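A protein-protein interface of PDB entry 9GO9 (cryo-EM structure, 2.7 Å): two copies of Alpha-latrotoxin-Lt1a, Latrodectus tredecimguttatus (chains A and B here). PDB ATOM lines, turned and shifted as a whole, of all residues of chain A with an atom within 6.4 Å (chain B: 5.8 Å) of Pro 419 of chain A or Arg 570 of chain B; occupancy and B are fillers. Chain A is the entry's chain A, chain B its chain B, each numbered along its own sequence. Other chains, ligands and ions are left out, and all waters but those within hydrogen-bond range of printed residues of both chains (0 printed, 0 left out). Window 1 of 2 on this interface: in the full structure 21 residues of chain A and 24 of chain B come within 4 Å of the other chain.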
ATOM      1  N   GLU A 360      30.070   7.312   2.678  1.00  0.00           N
ATOM      2  CA  GLU A 360      29.673   8.477   3.457  1.00  0.00           C
ATOM      3  C   GLU A 360      28.871   8.028   4.670  1.00  0.00           C
ATOM      4  O   GLU A 360      27.969   7.192   4.555  1.00  0.00           O
ATOM      5  CB  GLU A 360      28.848   9.450   2.612  1.00  0.00           C
ATOM      6  CG  GLU A 360      29.444   9.751   1.247  1.00  0.00           C
ATOM      7  CD  GLU A 360      30.810  10.403   1.337  1.00  0.00           C
ATOM      8  OE1 GLU A 360      30.959  11.373   2.109  1.00  0.00           O
ATOM      9  OE2 GLU A 360      31.736   9.945   0.635  1.00  0.00           O
ATOM     10  N   ASN A 361      29.200   8.586   5.832  1.00  0.00           N
ATOM     11  CA  ASN A 361      28.558   8.178   7.071  1.00  0.00           C
ATOM     12  C   ASN A 361      27.170   8.812   7.173  1.00  0.00           C
ATOM     13  O   ASN A 361      26.665   9.429   6.231  1.00  0.00           O
ATOM     14  CB  ASN A 361      29.431   8.555   8.265  1.00  0.00           C
ATOM     15  CG  ASN A 361      29.399   7.509   9.361  1.00  0.00           C
ATOM     16  OD1 ASN A 361      28.335   7.134   9.849  1.00  0.00           O
ATOM     17  ND2 ASN A 361      30.574   7.032   9.755  1.00  0.00           N
ATOM     18  N   PHE A 362      26.541   8.655   8.336  1.00  0.00           N
ATOM     19  CA  PHE A 362      25.184   9.156   8.517  1.00  0.00           C
ATOM     20  C   PHE A 362      25.168  10.679   8.496  1.00  0.00           C
ATOM     21  O   PHE A 362      26.119  11.335   8.930  1.00  0.00           O
ATOM     22  CB  PHE A 362      24.583   8.645   9.828  1.00  0.00           C
ATOM     23  CG  PHE A 362      25.230   9.208  11.064  1.00  0.00           C
ATOM     24  CD1 PHE A 362      26.393   8.654  11.571  1.00  0.00           C
ATOM     25  CD2 PHE A 362      24.667  10.288  11.726  1.00  0.00           C
ATOM     26  CE1 PHE A 362      26.986   9.170  12.706  1.00  0.00           C
ATOM     27  CE2 PHE A 362      25.256  10.808  12.861  1.00  0.00           C
ATOM     28  CZ  PHE A 362      26.416  10.248  13.352  1.00  0.00           C
ATOM     29  N   ALA A 363      24.076  11.241   7.980  1.00  0.00           N
ATOM     30  CA  ALA A 363      23.917  12.688   7.919  1.00  0.00           C
ATOM     31  C   ALA A 363      23.211  13.257   9.140  1.00  0.00           C
ATOM     32  O   ALA A 363      23.423  14.427   9.478  1.00  0.00           O
ATOM     33  CB  ALA A 363      23.149  13.082   6.655  1.00  0.00           C
ATOM     34  N   ARG A 417      19.827   8.667   9.597  1.00  0.00           N
ATOM     35  CA  ARG A 417      19.412   9.044   8.253  1.00  0.00           C
ATOM     36  C   ARG A 417      20.619   8.946   7.329  1.00  0.00           C
ATOM     37  O   ARG A 417      21.617   9.647   7.528  1.00  0.00           O
ATOM     38  CB  ARG A 417      18.831  10.458   8.245  1.00  0.00           C
ATOM     39  CG  ARG A 417      18.448  10.978   6.873  1.00  0.00           C
ATOM     40  CD  ARG A 417      17.695  12.291   6.991  1.00  0.00           C
ATOM     41  NE  ARG A 417      16.492  12.153   7.802  1.00  0.00           N
ATOM     42  CZ  ARG A 417      16.160  12.964   8.797  1.00  0.00           C
ATOM     43  NH1 ARG A 417      16.926  13.988   9.137  1.00  0.00           N
ATOM     44  NH2 ARG A 417      15.035  12.741   9.470  1.00  0.00           N
ATOM     45  N   MET A 418      20.526   8.078   6.325  1.00  0.00           N
ATOM     46  CA  MET A 418      21.656   7.785   5.458  1.00  0.00           C
ATOM     47  C   MET A 418      21.456   8.407   4.088  1.00  0.00           C
ATOM     48  O   MET A 418      20.395   8.220   3.477  1.00  0.00           O
ATOM     49  CB  MET A 418      21.845   6.269   5.318  1.00  0.00           C
ATOM     50  CG  MET A 418      22.197   5.566   6.620  1.00  0.00           C
ATOM     51  SD  MET A 418      23.943   5.693   7.055  1.00  0.00           S
ATOM     52  CE  MET A 418      24.706   5.690   5.434  1.00  0.00           C
ATOM     53  N   PRO A 419      22.434   9.150   3.578  1.00  0.00           N
ATOM     54  CA  PRO A 419      22.326   9.683   2.217  1.00  0.00           C
ATOM     55  C   PRO A 419      22.398   8.570   1.182  1.00  0.00           C
ATOM     56  O   PRO A 419      22.956   7.497   1.414  1.00  0.00           O
ATOM     57  CB  PRO A 419      23.531  10.627   2.099  1.00  0.00           C
ATOM     58  CG  PRO A 419      24.053  10.797   3.499  1.00  0.00           C
ATOM     59  CD  PRO A 419      23.689   9.550   4.231  1.00  0.00           C
ATOM     60  N   VAL A 420      21.810   8.847   0.017  1.00  0.00           N
ATOM     61  CA  VAL A 420      21.806   7.874  -1.067  1.00  0.00           C
ATOM     62  C   VAL A 420      23.221   7.705  -1.600  1.00  0.00           C
ATOM     63  O   VAL A 420      23.913   8.688  -1.896  1.00  0.00           O
ATOM     64  CB  VAL A 420      20.838   8.310  -2.177  1.00  0.00           C
ATOM     65  CG1 VAL A 420      20.997   7.425  -3.404  1.00  0.00           C
ATOM     66  CG2 VAL A 420      19.403   8.275  -1.671  1.00  0.00           C
ATOM     67  N   ASP A 421      23.660   6.455  -1.720  1.00  0.00           N
ATOM     68  CA  ASP A 421      25.011   6.173  -2.184  1.00  0.00           C
ATOM     69  C   ASP A 421      25.173   6.566  -3.647  1.00  0.00           C
ATOM     70  O   ASP A 421      24.298   6.309  -4.479  1.00  0.00           O
ATOM     71  CB  ASP A 421      25.337   4.692  -1.998  1.00  0.00           C
ATOM     72  CG  ASP A 421      26.820   4.405  -2.114  1.00  0.00           C
ATOM     73  OD1 ASP A 421      27.610   5.050  -1.394  1.00  0.00           O
ATOM     74  OD2 ASP A 421      27.197   3.533  -2.924  1.00  0.00           O
ATOM     75  N   GLN A 422      26.306   7.201  -3.956  1.00  0.00           N
ATOM     76  CA  GLN A 422      26.584   7.599  -5.332  1.00  0.00           C
ATOM     77  C   GLN A 422      26.748   6.388  -6.242  1.00  0.00           C
ATOM     78  O   GLN A 422      26.235   6.375  -7.366  1.00  0.00           O
ATOM     79  CB  GLN A 422      27.838   8.473  -5.377  1.00  0.00           C
ATOM     80  CG  GLN A 422      28.173   9.014  -6.755  1.00  0.00           C
ATOM     81  CD  GLN A 422      29.392   9.914  -6.745  1.00  0.00           C
ATOM     82  OE1 GLN A 422      30.023  10.113  -5.706  1.00  0.00           O
ATOM     83  NE2 GLN A 422      29.732  10.465  -7.904  1.00  0.00           N
ATOM     84  N   THR A 445      20.610  -0.571   2.315  1.00  0.00           N
ATOM     85  CA  THR A 445      20.421  -0.579   0.874  1.00  0.00           C
ATOM     86  C   THR A 445      20.548   0.829   0.310  1.00  0.00           C
ATOM     87  O   THR A 445      20.335   1.817   1.020  1.00  0.00           O
ATOM     88  CB  THR A 445      19.050  -1.159   0.531  1.00  0.00           C
ATOM     89  OG1 THR A 445      18.050  -0.547   1.355  1.00  0.00           O
ATOM     90  CG2 THR A 445      19.037  -2.663   0.762  1.00  0.00           C
ATOM     91  N   PRO A 446      20.905   0.956  -0.971  1.00  0.00           N
ATOM     92  CA  PRO A 446      21.077   2.298  -1.551  1.00  0.00           C
ATOM     93  C   PRO A 446      19.822   3.154  -1.526  1.00  0.00           C
ATOM     94  O   PRO A 446      19.930   4.385  -1.500  1.00  0.00           O
ATOM     95  CB  PRO A 446      21.517   1.997  -2.991  1.00  0.00           C
ATOM     96  CG  PRO A 446      22.154   0.656  -2.913  1.00  0.00           C
ATOM     97  CD  PRO A 446      21.359  -0.102  -1.891  1.00  0.00           C
ATOM     98  N   LEU A 448      17.128   3.069   0.696  1.00  0.00           N
ATOM     99  CA  LEU A 448      16.428   3.189   1.968  1.00  0.00           C
ATOM    100  C   LEU A 448      17.281   4.032   2.904  1.00  0.00           C
ATOM    101  O   LEU A 448      18.483   3.783   3.045  1.00  0.00           O
ATOM    102  CB  LEU A 448      16.135   1.808   2.574  1.00  0.00           C
ATOM    103  CG  LEU A 448      15.250   1.696   3.823  1.00  0.00           C
ATOM    104  CD1 LEU A 448      14.574   0.335   3.851  1.00  0.00           C
ATOM    105  CD2 LEU A 448      16.031   1.912   5.107  1.00  0.00           C
ATOM    106  N   SER A 449      16.660   5.026   3.539  1.00  0.00           N
ATOM    107  CA  SER A 449      17.381   6.010   4.342  1.00  0.00           C
ATOM    108  C   SER A 449      17.302   5.720   5.838  1.00  0.00           C
ATOM    109  O   SER A 449      18.335   5.601   6.505  1.00  0.00           O
ATOM    110  CB  SER A 449      16.844   7.417   4.044  1.00  0.00           C
ATOM    111  OG  SER A 449      15.500   7.549   4.472  1.00  0.00           O
ATOM    112  N   ALA B 534      17.968  21.956   5.481  1.00  0.00           N
ATOM    113  CA  ALA B 534      17.799  21.177   4.258  1.00  0.00           C
ATOM    114  C   ALA B 534      18.895  20.132   4.095  1.00  0.00           C
ATOM    115  O   ALA B 534      18.634  19.038   3.582  1.00  0.00           O
ATOM    116  CB  ALA B 534      17.770  22.106   3.044  1.00  0.00           C
ATOM    117  N   ASP B 535      20.121  20.443   4.522  1.00  0.00           N
ATOM    118  CA  ASP B 535      21.231  19.515   4.349  1.00  0.00           C
ATOM    119  C   ASP B 535      21.170  18.339   5.315  1.00  0.00           C
ATOM    120  O   ASP B 535      21.762  17.292   5.032  1.00  0.00           O
ATOM    121  CB  ASP B 535      22.560  20.254   4.513  1.00  0.00           C
ATOM    122  CG  ASP B 535      23.714  19.535   3.848  1.00  0.00           C
ATOM    123  OD1 ASP B 535      23.466  18.762   2.899  1.00  0.00           O
ATOM    124  OD2 ASP B 535      24.869  19.742   4.272  1.00  0.00           O
ATOM    125  N   SER B 536      20.478  18.484   6.442  1.00  0.00           N
ATOM    126  CA  SER B 536      20.381  17.419   7.432  1.00  0.00           C
ATOM    127  C   SER B 536      19.163  16.526   7.229  1.00  0.00           C
ATOM    128  O   SER B 536      19.000  15.552   7.969  1.00  0.00           O
ATOM    129  CB  SER B 536      20.352  18.012   8.845  1.00  0.00           C
ATOM    130  OG  SER B 536      19.171  18.765   9.060  1.00  0.00           O
ATOM    131  N   HIS B 565      19.861  22.618  -3.956  1.00  0.00           N
ATOM    132  CA  HIS B 565      21.051  21.864  -4.340  1.00  0.00           C
ATOM    133  C   HIS B 565      21.437  20.867  -3.255  1.00  0.00           C
ATOM    134  O   HIS B 565      21.745  19.705  -3.541  1.00  0.00           O
ATOM    135  CB  HIS B 565      22.211  22.818  -4.621  1.00  0.00           C
ATOM    136  CG  HIS B 565      22.026  23.660  -5.845  1.00  0.00           C
ATOM    137  ND1 HIS B 565      21.088  24.667  -5.920  1.00  0.00           N
ATOM    138  CD2 HIS B 565      22.665  23.652  -7.039  1.00  0.00           C
ATOM    139  CE1 HIS B 565      21.154  25.239  -7.109  1.00  0.00           C
ATOM    140  NE2 HIS B 565      22.103  24.642  -7.807  1.00  0.00           N
ATOM    141  N   LEU B 566      21.424  21.310  -1.995  1.00  0.00           N
ATOM    142  CA  LEU B 566      21.783  20.425  -0.892  1.00  0.00           C
ATOM    143  C   LEU B 566      20.770  19.299  -0.732  1.00  0.00           C
ATOM    144  O   LEU B 566      21.145  18.154  -0.455  1.00  0.00           O
ATOM    145  CB  LEU B 566      21.906  21.227   0.403  1.00  0.00           C
ATOM    146  CG  LEU B 566      22.910  22.381   0.387  1.00  0.00           C
ATOM    147  CD1 LEU B 566      22.969  23.058   1.746  1.00  0.00           C
ATOM    148  CD2 LEU B 566      24.287  21.890  -0.031  1.00  0.00           C
ATOM    149  N   ALA B 567      19.480  19.606  -0.891  1.00  0.00           N
ATOM    150  CA  ALA B 567      18.458  18.569  -0.789  1.00  0.00           C
ATOM    151  C   ALA B 567      18.592  17.544  -1.908  1.00  0.00           C
ATOM    152  O   ALA B 567      18.413  16.341  -1.680  1.00  0.00           O
ATOM    153  CB  ALA B 567      17.067  19.200  -0.801  1.00  0.00           C
ATOM    154  N   ALA B 568      18.904  17.997  -3.124  1.00  0.00           N
ATOM    155  CA  ALA B 568      19.013  17.086  -4.257  1.00  0.00           C
ATOM    156  C   ALA B 568      20.295  16.264  -4.222  1.00  0.00           C
ATOM    157  O   ALA B 568      20.297  15.115  -4.678  1.00  0.00           O
ATOM    158  CB  ALA B 568      18.932  17.868  -5.569  1.00  0.00           C
ATOM    159  N   GLN B 569      21.387  16.823  -3.695  1.00  0.00           N
ATOM    160  CA  GLN B 569      22.654  16.103  -3.677  1.00  0.00           C
ATOM    161  C   GLN B 569      22.622  14.882  -2.766  1.00  0.00           C
ATOM    162  O   GLN B 569      23.403  13.949  -2.977  1.00  0.00           O
ATOM    163  CB  GLN B 569      23.783  17.042  -3.249  1.00  0.00           C
ATOM    164  CG  GLN B 569      25.147  16.665  -3.798  1.00  0.00           C
ATOM    165  CD  GLN B 569      26.267  17.476  -3.177  1.00  0.00           C
ATOM    166  OE1 GLN B 569      26.098  18.072  -2.114  1.00  0.00           O
ATOM    167  NE2 GLN B 569      27.417  17.500  -3.839  1.00  0.00           N
ATOM    168  N   ARG B 570      21.743  14.865  -1.765  1.00  0.00           N
ATOM    169  CA  ARG B 570      21.651  13.739  -0.846  1.00  0.00           C
ATOM    170  C   ARG B 570      20.473  12.819  -1.131  1.00  0.00           C
ATOM    171  O   ARG B 570      20.545  11.630  -0.801  1.00  0.00           O
ATOM    172  CB  ARG B 570      21.559  14.239   0.601  1.00  0.00           C
ATOM    173  CG  ARG B 570      22.823  14.920   1.103  1.00  0.00           C
ATOM    174  CD  ARG B 570      22.675  15.359   2.550  1.00  0.00           C
ATOM    175  NE  ARG B 570      23.844  16.091   3.022  1.00  0.00           N
ATOM    176  CZ  ARG B 570      24.907  15.527   3.577  1.00  0.00           C
ATOM    177  NH1 ARG B 570      24.985  14.218   3.751  1.00  0.00           N
ATOM    178  NH2 ARG B 570      25.920  16.295   3.969  1.00  0.00           N
ATOM    179  N   GLY B 571      19.403  13.328  -1.725  1.00  0.00           N
ATOM    180  CA  GLY B 571      18.260  12.519  -2.075  1.00  0.00           C
ATOM    181  C   GLY B 571      17.138  12.484  -1.063  1.00  0.00           C
ATOM    182  O   GLY B 571      16.621  11.398  -0.780  1.00  0.00           O
ATOM    183  N   PHE B 572      16.741  13.628  -0.513  1.00  0.00           N
ATOM    184  CA  PHE B 572      15.641  13.688   0.439  1.00  0.00           C
ATOM    185  C   PHE B 572      14.401  14.240  -0.252  1.00  0.00           C
ATOM    186  O   PHE B 572      14.450  15.308  -0.872  1.00  0.00           O
ATOM    187  CB  PHE B 572      16.014  14.553   1.643  1.00  0.00           C
ATOM    188  CG  PHE B 572      17.219  14.061   2.392  1.00  0.00           C
ATOM    189  CD1 PHE B 572      17.326  12.730   2.761  1.00  0.00           C
ATOM    190  CD2 PHE B 572      18.245  14.927   2.728  1.00  0.00           C
ATOM    191  CE1 PHE B 572      18.434  12.273   3.449  1.00  0.00           C
ATOM    192  CE2 PHE B 572      19.355  14.476   3.417  1.00  0.00           C
ATOM    193  CZ  PHE B 572      19.449  13.148   3.777  1.00  0.00           C
ATOM    194  N   ARG B 603      22.798  12.380  -8.480  1.00  0.00           N
ATOM    195  CA  ARG B 603      23.242  11.625  -7.311  1.00  0.00           C
ATOM    196  C   ARG B 603      22.084  10.872  -6.666  1.00  0.00           C
ATOM    197  O   ARG B 603      22.228   9.703  -6.290  1.00  0.00           O
ATOM    198  CB  ARG B 603      23.900  12.564  -6.301  1.00  0.00           C
ATOM    199  CG  ARG B 603      25.417  12.591  -6.375  1.00  0.00           C
ATOM    200  CD  ARG B 603      26.020  13.142  -5.094  1.00  0.00           C
ATOM    201  NE  ARG B 603      27.474  13.024  -5.080  1.00  0.00           N
ATOM    202  CZ  ARG B 603      28.212  13.003  -3.980  1.00  0.00           C
ATOM    203  NH1 ARG B 603      27.665  13.089  -2.778  1.00  0.00           N
ATOM    204  NH2 ARG B 603      29.533  12.892  -4.087  1.00  0.00           N
ATOM    205  N   GLY B 604      20.932  11.523  -6.527  1.00  0.00           N
ATOM    206  CA  GLY B 604      19.736  10.838  -6.083  1.00  0.00           C
ATOM    207  C   GLY B 604      19.266   9.833  -7.115  1.00  0.00           C
ATOM    208  O   GLY B 604      19.172  10.158  -8.302  1.00  0.00           O
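Of chain B, only Arg 570 comes within 4 Å of Pro 419 of chain A.
Of chain A, only Ala 363, Pro 419 and Val 420 come within 4 Å of Arg 570 of chain B.
Of the printed residues of chain B, Ala 363 of chain A touches Arg 570.
Of the printed residues of chain A, Arg 603 of chain B touches Val 420 and Gln 422.
Thr 445 of chain A touches none of the printed residues of chain B.
NH1 of Arg 417 of chain A is in hydrogen-bond range of O of Ser 536 of chain B.
N of Val 420 of chain A sits at hydrogen-bond distance from O of Arg 570 of chain B (3.2 Å).
The side-chain amide oxygen (OE1) of Gln 422 of chain A is in hydrogen-bond range of the guanidinium group (NH2) of Arg 603 of chain B (3.3 Å).
Among the printed residues, merely in contact across the chains: Ala 363 of chain A with Arg 570 of chain B, Arg 417 of chain A with Phe 572 of chain B, Pro 419 of chain A with Arg 570 of chain B and Val 420 of chain A with Arg 603 of chain B.
Of the 14 printed residues of chain A, 5 touch a printed residue of chain B.
Hydrophobic or aromatic side chains of chain B within 4 Å of the printed part of chain A: Phe 572.
Among the printed residues, no Asp or Glu carboxylate lies within 4 Å of a Lys or Arg side-chain nitrogen of the other chain.
No position is printed for both chains.
The backbone carbonyl oxygen (O) of Arg 417 of chain A is in hydrogen-bond range of the backbone NH (N) of Ala 363 of chain A, at 3.0 Å.
O of Ala 567 of chain B is in hydrogen-bond range of N of Phe 572 of chain B (3.4 Å).
OD1 of Asp 535 of chain B is in salt-bridge range of NE of Arg 570 of chain B.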
